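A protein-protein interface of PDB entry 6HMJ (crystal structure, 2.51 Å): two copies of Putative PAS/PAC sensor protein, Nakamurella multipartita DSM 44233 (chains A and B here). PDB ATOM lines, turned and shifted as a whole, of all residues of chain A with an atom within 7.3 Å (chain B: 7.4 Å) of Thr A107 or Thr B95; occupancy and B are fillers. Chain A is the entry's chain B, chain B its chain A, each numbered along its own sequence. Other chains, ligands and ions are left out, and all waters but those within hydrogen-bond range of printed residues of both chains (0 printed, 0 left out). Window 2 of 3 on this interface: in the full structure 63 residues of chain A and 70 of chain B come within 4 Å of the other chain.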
ATOM      1  N   SER A  14      23.862  33.667  18.484  1.00  0.00           N
ATOM      2  CA  SER A  14      23.236  32.687  19.355  1.00  0.00           C
ATOM      3  C   SER A  14      24.156  32.339  20.514  1.00  0.00           C
ATOM      4  O   SER A  14      25.379  32.472  20.424  1.00  0.00           O
ATOM      5  CB  SER A  14      22.879  31.409  18.582  1.00  0.00           C
ATOM      6  OG  SER A  14      24.048  30.738  18.143  1.00  0.00           O
ATOM      7  N   PHE A  15      23.544  31.893  21.610  1.00  0.00           N
ATOM      8  CA  PHE A  15      24.275  31.374  22.755  1.00  0.00           C
ATOM      9  C   PHE A  15      23.438  30.279  23.399  1.00  0.00           C
ATOM     10  O   PHE A  15      22.250  30.120  23.104  1.00  0.00           O
ATOM     11  CB  PHE A  15      24.611  32.473  23.773  1.00  0.00           C
ATOM     12  CG  PHE A  15      23.406  33.126  24.400  1.00  0.00           C
ATOM     13  CD1 PHE A  15      22.690  32.485  25.402  1.00  0.00           C
ATOM     14  CD2 PHE A  15      23.012  34.398  24.016  1.00  0.00           C
ATOM     15  CE1 PHE A  15      21.590  33.085  25.983  1.00  0.00           C
ATOM     16  CE2 PHE A  15      21.913  35.006  24.599  1.00  0.00           C
ATOM     17  CZ  PHE A  15      21.204  34.349  25.586  1.00  0.00           C
ATOM     18  N   VAL A  16      24.071  29.520  24.289  1.00  0.00           N
ATOM     19  CA  VAL A  16      23.394  28.469  25.038  1.00  0.00           C
ATOM     20  C   VAL A  16      23.942  28.448  26.457  1.00  0.00           C
ATOM     21  O   VAL A  16      25.155  28.547  26.666  1.00  0.00           O
ATOM     22  CB  VAL A  16      23.570  27.092  24.362  1.00  0.00           C
ATOM     23  CG1 VAL A  16      22.989  25.988  25.234  1.00  0.00           C
ATOM     24  CG2 VAL A  16      22.933  27.096  22.981  1.00  0.00           C
ATOM     25  N   LEU A  17      23.046  28.313  27.434  1.00  0.00           N
ATOM     26  CA  LEU A  17      23.417  28.214  28.840  1.00  0.00           C
ATOM     27  C   LEU A  17      22.841  26.938  29.433  1.00  0.00           C
ATOM     28  O   LEU A  17      21.647  26.660  29.275  1.00  0.00           O
ATOM     29  CB  LEU A  17      22.920  29.424  29.639  1.00  0.00           C
ATOM     30  CG  LEU A  17      23.386  29.457  31.100  1.00  0.00           C
ATOM     31  CD1 LEU A  17      24.897  29.637  31.194  1.00  0.00           C
ATOM     32  CD2 LEU A  17      22.663  30.542  31.882  1.00  0.00           C
ATOM     33  N   LEU A  64      15.981  36.084  31.198  1.00  0.00           N
ATOM     34  CA  LEU A  64      16.668  34.799  31.224  1.00  0.00           C
ATOM     35  C   LEU A  64      16.283  33.997  32.462  1.00  0.00           C
ATOM     36  O   LEU A  64      15.983  32.802  32.370  1.00  0.00           O
ATOM     37  CB  LEU A  64      18.178  35.016  31.166  1.00  0.00           C
ATOM     38  CG  LEU A  64      19.040  33.753  31.249  1.00  0.00           C
ATOM     39  CD1 LEU A  64      18.613  32.730  30.208  1.00  0.00           C
ATOM     40  CD2 LEU A  64      20.508  34.105  31.080  1.00  0.00           C
ATOM     41  N   CYS A  67      12.919  32.416  32.079  1.00  0.00           N
ATOM     42  CA  CYS A  67      12.936  31.298  31.142  1.00  0.00           C
ATOM     43  C   CYS A  67      13.499  30.044  31.795  1.00  0.00           C
ATOM     44  O   CYS A  67      13.053  28.932  31.494  1.00  0.00           O
ATOM     45  CB  CYS A  67      13.755  31.661  29.904  1.00  0.00           C
ATOM     46  SG  CYS A  67      13.657  30.447  28.557  1.00  0.00           S
ATOM     47  N   VAL A  74      10.810  33.623  26.162  1.00  0.00           N
ATOM     48  CA  VAL A  74      10.841  35.024  26.555  1.00  0.00           C
ATOM     49  C   VAL A  74      11.389  35.848  25.401  1.00  0.00           C
ATOM     50  O   VAL A  74      12.261  35.400  24.651  1.00  0.00           O
ATOM     51  CB  VAL A  74      11.698  35.242  27.823  1.00  0.00           C
ATOM     52  CG1 VAL A  74      11.578  36.680  28.304  1.00  0.00           C
ATOM     53  CG2 VAL A  74      11.290  34.270  28.921  1.00  0.00           C
ATOM     54  N   THR A  92      16.043  39.994  21.700  1.00  0.00           N
ATOM     55  CA  THR A  92      16.552  38.707  22.152  1.00  0.00           C
ATOM     56  C   THR A  92      15.384  37.771  22.417  1.00  0.00           C
ATOM     57  O   THR A  92      14.482  38.105  23.192  1.00  0.00           O
ATOM     58  CB  THR A  92      17.403  38.859  23.416  1.00  0.00           C
ATOM     59  OG1 THR A  92      18.650  39.480  23.083  1.00  0.00           O
ATOM     60  CG2 THR A  92      17.670  37.503  24.049  1.00  0.00           C
ATOM     61  N   THR A  93      15.403  36.603  21.781  1.00  0.00           N
ATOM     62  CA  THR A  93      14.437  35.549  22.048  1.00  0.00           C
ATOM     63  C   THR A  93      15.121  34.434  22.828  1.00  0.00           C
ATOM     64  O   THR A  93      16.284  34.109  22.570  1.00  0.00           O
ATOM     65  CB  THR A  93      13.839  34.995  20.753  1.00  0.00           C
ATOM     66  OG1 THR A  93      14.825  34.225  20.062  1.00  0.00           O
ATOM     67  CG2 THR A  93      13.360  36.130  19.854  1.00  0.00           C
ATOM     68  N   LEU A  94      14.400  33.862  23.790  1.00  0.00           N
ATOM     69  CA  LEU A  94      14.923  32.810  24.651  1.00  0.00           C
ATOM     70  C   LEU A  94      13.954  31.638  24.652  1.00  0.00           C
ATOM     71  O   LEU A  94      12.740  31.835  24.762  1.00  0.00           O
ATOM     72  CB  LEU A  94      15.132  33.303  26.087  1.00  0.00           C
ATOM     73  CG  LEU A  94      16.114  34.445  26.334  1.00  0.00           C
ATOM     74  CD1 LEU A  94      15.965  34.936  27.762  1.00  0.00           C
ATOM     75  CD2 LEU A  94      17.539  33.995  26.073  1.00  0.00           C
ATOM     76  N   THR A  95      14.490  30.427  24.520  1.00  0.00           N
ATOM     77  CA  THR A  95      13.703  29.208  24.616  1.00  0.00           C
ATOM     78  C   THR A  95      14.440  28.215  25.504  1.00  0.00           C
ATOM     79  O   THR A  95      15.664  28.276  25.656  1.00  0.00           O
ATOM     80  CB  THR A  95      13.440  28.587  23.237  1.00  0.00           C
ATOM     81  OG1 THR A  95      14.684  28.387  22.554  1.00  0.00           O
ATOM     82  CG2 THR A  95      12.543  29.491  22.401  1.00  0.00           C
ATOM     83  N   ALA A  96      13.677  27.302  26.099  1.00  0.00           N
ATOM     84  CA  ALA A  96      14.196  26.374  27.092  1.00  0.00           C
ATOM     85  C   ALA A  96      13.960  24.933  26.662  1.00  0.00           C
ATOM     86  O   ALA A  96      13.038  24.636  25.895  1.00  0.00           O
ATOM     87  CB  ALA A  96      13.546  26.614  28.463  1.00  0.00           C
ATOM     88  N   LEU A  97      14.806  24.040  27.169  1.00  0.00           N
ATOM     89  CA  LEU A  97      14.630  22.599  27.031  1.00  0.00           C
ATOM     90  C   LEU A  97      14.286  22.028  28.402  1.00  0.00           C
ATOM     91  O   LEU A  97      15.067  22.175  29.349  1.00  0.00           O
ATOM     92  CB  LEU A  97      15.882  21.935  26.462  1.00  0.00           C
ATOM     93  CG  LEU A  97      15.895  20.405  26.531  1.00  0.00           C
ATOM     94  CD1 LEU A  97      14.665  19.829  25.841  1.00  0.00           C
ATOM     95  CD2 LEU A  97      17.164  19.852  25.904  1.00  0.00           C
ATOM     96  N   ALA A 105      18.664  23.561  29.761  1.00  0.00           N
ATOM     97  CA  ALA A 105      19.480  24.562  29.089  1.00  0.00           C
ATOM     98  C   ALA A 105      18.580  25.572  28.393  1.00  0.00           C
ATOM     99  O   ALA A 105      17.442  25.264  28.029  1.00  0.00           O
ATOM    100  CB  ALA A 105      20.432  23.915  28.076  1.00  0.00           C
ATOM    101  N   VAL A 106      19.110  26.782  28.216  1.00  0.00           N
ATOM    102  CA  VAL A 106      18.423  27.863  27.520  1.00  0.00           C
ATOM    103  C   VAL A 106      19.270  28.288  26.328  1.00  0.00           C
ATOM    104  O   VAL A 106      20.472  28.543  26.474  1.00  0.00           O
ATOM    105  CB  VAL A 106      18.163  29.065  28.446  1.00  0.00           C
ATOM    106  CG1 VAL A 106      17.644  30.255  27.647  1.00  0.00           C
ATOM    107  CG2 VAL A 106      17.171  28.692  29.535  1.00  0.00           C
ATOM    108  N   THR A 107      18.642  28.374  25.159  1.00  0.00           N
ATOM    109  CA  THR A 107      19.281  28.896  23.959  1.00  0.00           C
ATOM    110  C   THR A 107      18.701  30.273  23.662  1.00  0.00           C
ATOM    111  O   THR A 107      17.476  30.444  23.647  1.00  0.00           O
ATOM    112  CB  THR A 107      19.081  27.962  22.761  1.00  0.00           C
ATOM    113  OG1 THR A 107      17.762  28.129  22.227  1.00  0.00           O
ATOM    114  CG2 THR A 107      19.276  26.506  23.170  1.00  0.00           C
ATOM    115  N   GLY A 108      19.578  31.246  23.437  1.00  0.00           N
ATOM    116  CA  GLY A 108      19.165  32.606  23.157  1.00  0.00           C
ATOM    117  C   GLY A 108      19.643  33.052  21.789  1.00  0.00           C
ATOM    118  O   GLY A 108      20.663  32.577  21.287  1.00  0.00           O
ATOM    119  N   VAL A 109      18.895  33.973  21.189  1.00  0.00           N
ATOM    120  CA  VAL A 109      19.211  34.513  19.871  1.00  0.00           C
ATOM    121  C   VAL A 109      19.066  36.026  19.942  1.00  0.00           C
ATOM    122  O   VAL A 109      17.953  36.540  20.100  1.00  0.00           O
ATOM    123  CB  VAL A 109      18.311  33.930  18.771  1.00  0.00           C
ATOM    124  CG1 VAL A 109      18.573  34.630  17.440  1.00  0.00           C
ATOM    125  CG2 VAL A 109      18.534  32.433  18.643  1.00  0.00           C
ATOM    126  N   PHE B  15       6.160  27.847  18.743  1.00  0.00           N
ATOM    127  CA  PHE B  15       5.733  26.506  18.376  1.00  0.00           C
ATOM    128  C   PHE B  15       6.914  25.556  18.510  1.00  0.00           C
ATOM    129  O   PHE B  15       8.076  25.972  18.533  1.00  0.00           O
ATOM    130  CB  PHE B  15       5.160  26.443  16.950  1.00  0.00           C
ATOM    131  CG  PHE B  15       6.163  26.742  15.859  1.00  0.00           C
ATOM    132  CD1 PHE B  15       7.153  25.825  15.528  1.00  0.00           C
ATOM    133  CD2 PHE B  15       6.089  27.920  15.136  1.00  0.00           C
ATOM    134  CE1 PHE B  15       8.062  26.092  14.524  1.00  0.00           C
ATOM    135  CE2 PHE B  15       6.996  28.189  14.125  1.00  0.00           C
ATOM    136  CZ  PHE B  15       7.982  27.273  13.820  1.00  0.00           C
ATOM    137  N   VAL B  16       6.596  24.268  18.593  1.00  0.00           N
ATOM    138  CA  VAL B  16       7.594  23.207  18.587  1.00  0.00           C
ATOM    139  C   VAL B  16       7.182  22.195  17.528  1.00  0.00           C
ATOM    140  O   VAL B  16       6.009  21.809  17.453  1.00  0.00           O
ATOM    141  CB  VAL B  16       7.740  22.531  19.962  1.00  0.00           C
ATOM    142  CG1 VAL B  16       8.871  21.511  19.934  1.00  0.00           C
ATOM    143  CG2 VAL B  16       7.989  23.572  21.042  1.00  0.00           C
ATOM    144  N   CYS B  67      17.099  24.640   9.661  1.00  0.00           N
ATOM    145  CA  CYS B  67      17.320  24.430  11.088  1.00  0.00           C
ATOM    146  C   CYS B  67      17.172  22.963  11.462  1.00  0.00           C
ATOM    147  O   CYS B  67      17.853  22.483  12.376  1.00  0.00           O
ATOM    148  CB  CYS B  67      16.347  25.284  11.904  1.00  0.00           C
ATOM    149  SG  CYS B  67      16.638  25.257  13.697  1.00  0.00           S
ATOM    150  N   GLY B  71      20.582  22.118  12.434  1.00  0.00           N
ATOM    151  CA  GLY B  71      20.544  22.322  13.866  1.00  0.00           C
ATOM    152  C   GLY B  71      21.058  23.670  14.317  1.00  0.00           C
ATOM    153  O   GLY B  71      21.099  23.929  15.527  1.00  0.00           O
ATOM    154  N   ARG B  72      21.447  24.533  13.385  1.00  0.00           N
ATOM    155  CA  ARG B  72      21.987  25.874  13.546  1.00  0.00           C
ATOM    156  C   ARG B  72      20.839  26.878  13.635  1.00  0.00           C
ATOM    157  O   ARG B  72      19.860  26.761  12.893  1.00  0.00           O
ATOM    158  CB  ARG B  72      22.863  26.200  12.339  1.00  0.00           C
ATOM    159  CG  ARG B  72      24.087  25.294  12.202  1.00  0.00           C
ATOM    160  CD  ARG B  72      24.820  25.533  10.886  1.00  0.00           C
ATOM    161  NE  ARG B  72      25.995  24.678  10.736  1.00  0.00           N
ATOM    162  CZ  ARG B  72      26.769  24.649   9.654  1.00  0.00           C
ATOM    163  NH1 ARG B  72      26.486  25.416   8.609  1.00  0.00           N
ATOM    164  NH2 ARG B  72      27.819  23.839   9.606  1.00  0.00           N
ATOM    165  N   PRO B  73      20.897  27.877  14.518  1.00  0.00           N
ATOM    166  CA  PRO B  73      19.784  28.829  14.607  1.00  0.00           C
ATOM    167  C   PRO B  73      19.556  29.556  13.289  1.00  0.00           C
ATOM    168  O   PRO B  73      20.481  29.771  12.503  1.00  0.00           O
ATOM    169  CB  PRO B  73      20.230  29.791  15.712  1.00  0.00           C
ATOM    170  CG  PRO B  73      21.093  28.954  16.586  1.00  0.00           C
ATOM    171  CD  PRO B  73      21.818  28.010  15.662  1.00  0.00           C
ATOM    172  N   VAL B  74      18.302  29.940  13.059  1.00  0.00           N
ATOM    173  CA  VAL B  74      17.902  30.620  11.832  1.00  0.00           C
ATOM    174  C   VAL B  74      16.929  31.735  12.182  1.00  0.00           C
ATOM    175  O   VAL B  74      16.090  31.584  13.077  1.00  0.00           O
ATOM    176  CB  VAL B  74      17.254  29.642  10.828  1.00  0.00           C
ATOM    177  CG1 VAL B  74      16.932  30.353   9.522  1.00  0.00           C
ATOM    178  CG2 VAL B  74      18.158  28.439  10.589  1.00  0.00           C
ATOM    179  N   THR B  93      12.259  33.276  14.794  1.00  0.00           N
ATOM    180  CA  THR B  93      13.510  32.683  15.237  1.00  0.00           C
ATOM    181  C   THR B  93      13.306  31.184  15.412  1.00  0.00           C
ATOM    182  O   THR B  93      12.297  30.748  15.976  1.00  0.00           O
ATOM    183  CB  THR B  93      13.986  33.310  16.550  1.00  0.00           C
ATOM    184  OG1 THR B  93      14.137  34.725  16.379  1.00  0.00           O
ATOM    185  CG2 THR B  93      15.316  32.714  16.983  1.00  0.00           C
ATOM    186  N   LEU B  94      14.272  30.401  14.939  1.00  0.00           N
ATOM    187  CA  LEU B  94      14.182  28.947  14.961  1.00  0.00           C
ATOM    188  C   LEU B  94      15.426  28.391  15.635  1.00  0.00           C
ATOM    189  O   LEU B  94      16.547  28.674  15.200  1.00  0.00           O
ATOM    190  CB  LEU B  94      14.041  28.383  13.543  1.00  0.00           C
ATOM    191  CG  LEU B  94      12.876  28.918  12.708  1.00  0.00           C
ATOM    192  CD1 LEU B  94      13.127  28.660  11.232  1.00  0.00           C
ATOM    193  CD2 LEU B  94      11.557  28.297  13.139  1.00  0.00           C
ATOM    194  N   THR B  95      15.226  27.611  16.692  1.00  0.00           N
ATOM    195  CA  THR B  95      16.306  26.905  17.365  1.00  0.00           C
ATOM    196  C   THR B  95      15.946  25.430  17.473  1.00  0.00           C
ATOM    197  O   THR B  95      14.777  25.067  17.636  1.00  0.00           O
ATOM    198  CB  THR B  95      16.592  27.487  18.754  1.00  0.00           C
ATOM    199  OG1 THR B  95      15.383  27.544  19.516  1.00  0.00           O
ATOM    200  CG2 THR B  95      17.172  28.886  18.626  1.00  0.00           C
ATOM    201  N   ALA B  96      16.966  24.583  17.379  1.00  0.00           N
ATOM    202  CA  ALA B  96      16.794  23.140  17.369  1.00  0.00           C
ATOM    203  C   ALA B  96      17.175  22.539  18.715  1.00  0.00           C
ATOM    204  O   ALA B  96      18.101  23.011  19.385  1.00  0.00           O
ATOM    205  CB  ALA B  96      17.638  22.500  16.263  1.00  0.00           C
ATOM    206  N   LEU B  97      16.454  21.492  19.100  1.00  0.00           N
ATOM    207  CA  LEU B  97      16.696  20.776  20.346  1.00  0.00           C
ATOM    208  C   LEU B  97      17.447  19.495  20.002  1.00  0.00           C
ATOM    209  O   LEU B  97      16.870  18.560  19.435  1.00  0.00           O
ATOM    210  CB  LEU B  97      15.384  20.464  21.064  1.00  0.00           C
ATOM    211  CG  LEU B  97      14.527  21.644  21.527  1.00  0.00           C
ATOM    212  CD1 LEU B  97      13.175  21.149  22.024  1.00  0.00           C
ATOM    213  CD2 LEU B  97      15.232  22.440  22.613  1.00  0.00           C
ATOM    214  N   THR B  98      18.732  19.459  20.337  1.00  0.00           N
ATOM    215  CA  THR B  98      19.599  18.360  19.933  1.00  0.00           C
ATOM    216  C   THR B  98      19.425  17.160  20.857  1.00  0.00           C
ATOM    217  O   THR B  98      20.336  16.344  21.009  1.00  0.00           O
ATOM    218  CB  THR B  98      21.079  18.784  19.930  1.00  0.00           C
ATOM    219  OG1 THR B  98      21.588  18.763  21.269  1.00  0.00           O
ATOM    220  CG2 THR B  98      21.236  20.186  19.354  1.00  0.00           C
ATOM    221  N   VAL B 103      18.642  16.464  15.340  1.00  0.00           N
ATOM    222  CA  VAL B 103      17.571  17.413  15.625  1.00  0.00           C
ATOM    223  C   VAL B 103      16.342  16.631  16.071  1.00  0.00           C
ATOM    224  O   VAL B 103      15.785  15.833  15.309  1.00  0.00           O
ATOM    225  CB  VAL B 103      17.254  18.296  14.409  1.00  0.00           C
ATOM    226  CG1 VAL B 103      16.759  17.457  13.229  1.00  0.00           C
ATOM    227  CG2 VAL B 103      16.231  19.358  14.791  1.00  0.00           C
ATOM    228  N   ALA B 105      13.589  18.267  17.593  1.00  0.00           N
ATOM    229  CA  ALA B 105      12.490  19.158  17.245  1.00  0.00           C
ATOM    230  C   ALA B 105      13.078  20.550  17.048  1.00  0.00           C
ATOM    231  O   ALA B 105      14.225  20.818  17.417  1.00  0.00           O
ATOM    232  CB  ALA B 105      11.393  19.159  18.312  1.00  0.00           C
ATOM    233  N   VAL B 106      12.279  21.436  16.461  1.00  0.00           N
ATOM    234  CA  VAL B 106      12.659  22.829  16.258  1.00  0.00           C
ATOM    235  C   VAL B 106      11.677  23.707  17.018  1.00  0.00           C
ATOM    236  O   VAL B 106      10.459  23.583  16.843  1.00  0.00           O
ATOM    237  CB  VAL B 106      12.689  23.215  14.768  1.00  0.00           C
ATOM    238  CG1 VAL B 106      12.743  24.732  14.610  1.00  0.00           C
ATOM    239  CG2 VAL B 106      13.891  22.589  14.087  1.00  0.00           C
ATOM    240  N   THR B 107      12.210  24.594  17.853  1.00  0.00           N
ATOM    241  CA  THR B 107      11.403  25.587  18.545  1.00  0.00           C
ATOM    242  C   THR B 107      11.392  26.865  17.720  1.00  0.00           C
ATOM    243  O   THR B 107      12.450  27.386  17.353  1.00  0.00           O
ATOM    244  CB  THR B 107      11.950  25.868  19.945  1.00  0.00           C
ATOM    245  OG1 THR B 107      12.113  24.637  20.661  1.00  0.00           O
ATOM    246  CG2 THR B 107      11.001  26.769  20.716  1.00  0.00           C
ATOM    247  N   GLY B 108      10.195  27.360  17.430  1.00  0.00           N
ATOM    248  CA  GLY B 108      10.021  28.589  16.680  1.00  0.00           C
ATOM    249  C   GLY B 108       9.422  29.665  17.563  1.00  0.00           C
ATOM    250  O   GLY B 108       8.630  29.379  18.463  1.00  0.00           O
ATOM    251  N   VAL B 109       9.819  30.908  17.309  1.00  0.00           N
ATOM    252  CA  VAL B 109       9.277  32.067  18.005  1.00  0.00           C
ATOM    253  C   VAL B 109       8.926  33.089  16.935  1.00  0.00           C
ATOM    254  O   VAL B 109       9.820  33.632  16.273  1.00  0.00           O
ATOM    255  CB  VAL B 109      10.266  32.656  19.021  1.00  0.00           C
ATOM    256  CG1 VAL B 109       9.675  33.895  19.680  1.00  0.00           C
ATOM    257  CG2 VAL B 109      10.643  31.617  20.065  1.00  0.00           C
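Printed residues of chain B within 4 Å of Ser A14: Pro B73 (3.6 Å).
Printed residues of chain B within 4 Å of Leu A97: Leu B97.
Val A106 touches none of the printed residues of chain B.
Of chain B, only Thr B95 (3.7 Å) comes within 4 Å of Thr A107.
Phe B15 touches none of the printed residues of chain A.
Of the printed residues of chain A, Pro B73 touches Ser A14.
Thr B95 touches just these residues of chain A: Thr A95, Thr A107 and Val A109.
Of the printed residues of chain A, Leu B97 touches Leu A97 (3.9 Å).
The nearest residue of chain B that does not touch Thr A107 is Ala B96 (5.3 Å).
The nearest residue of chain A that does not touch Thr B95 is Gly A108 (5.7 Å).
The nearest printed residue of chain A that does not touch Pro B73 is Val A109 (4.3 Å).
Among the printed residues, merely in contact across the chains: Ser A14 with Pro B73, Thr A93 with Thr B93, Thr A95 with Thr B107, Thr A95 with Val B109, Leu A97 with Leu B97, Thr A107 with Thr B95, Val A109 with Thr B93 and Val A109 with Thr B95.
The side-chain hydroxyl (OG1) of Thr B95 is in hydrogen-bond range of the side-chain hydroxyl (OG1) of Thr A95 (3.2 Å).
The backbone NH (N) of Val B109 lies within hydrogen-bond range of the backbone carbonyl oxygen (O) of Thr B93 (2.8 Å).
O of Thr B95 lies within hydrogen-bond range of N of Thr B107 (2.6 Å).
The backbone carbonyl oxygen (O) of Ala B105 sits at hydrogen-bond distance from the backbone NH (N) of Leu B97 (2.9 Å).
The backbone carbonyl oxygen (O) of Thr A93 sits at hydrogen-bond distance from the backbone NH (N) of Val A109 (3.0 Å).
O of Thr A95 sits at hydrogen-bond distance from N of Thr A107, at 3.0 Å.
N of Leu A97 sits at hydrogen-bond distance from O of Ala A105 (3.0 Å).
Thr B93 touches its own counterpart, Thr A93.
Thr A95 touches Thr B107, and with the chains exchanged Thr A107 touches Thr B95.
Thr A95 touches Val B109, and with the chains exchanged Val A109 touches Thr B95.
Val A109 touches Thr B93, but with the chains exchanged Thr A93 does not touch Val B109 (4.3 Å).
Of the 19 printed residues of chain B, 6 touch a printed residue of chain A.
Of the 18 printed residues of chain A, 6 touch a printed residue of chain B.
Printed residues of chain A that touch a printed residue of chain B: Ser A14, Thr A93, Thr A95, Leu A97, Thr A107 and Val A109.
Hydrophobic or aromatic side chains of chain A within 4 Å of the printed part of chain B: Leu A97 and Val A109.
Along chain A the printed residues that touch a printed residue of chain B span positions 14 to 109.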
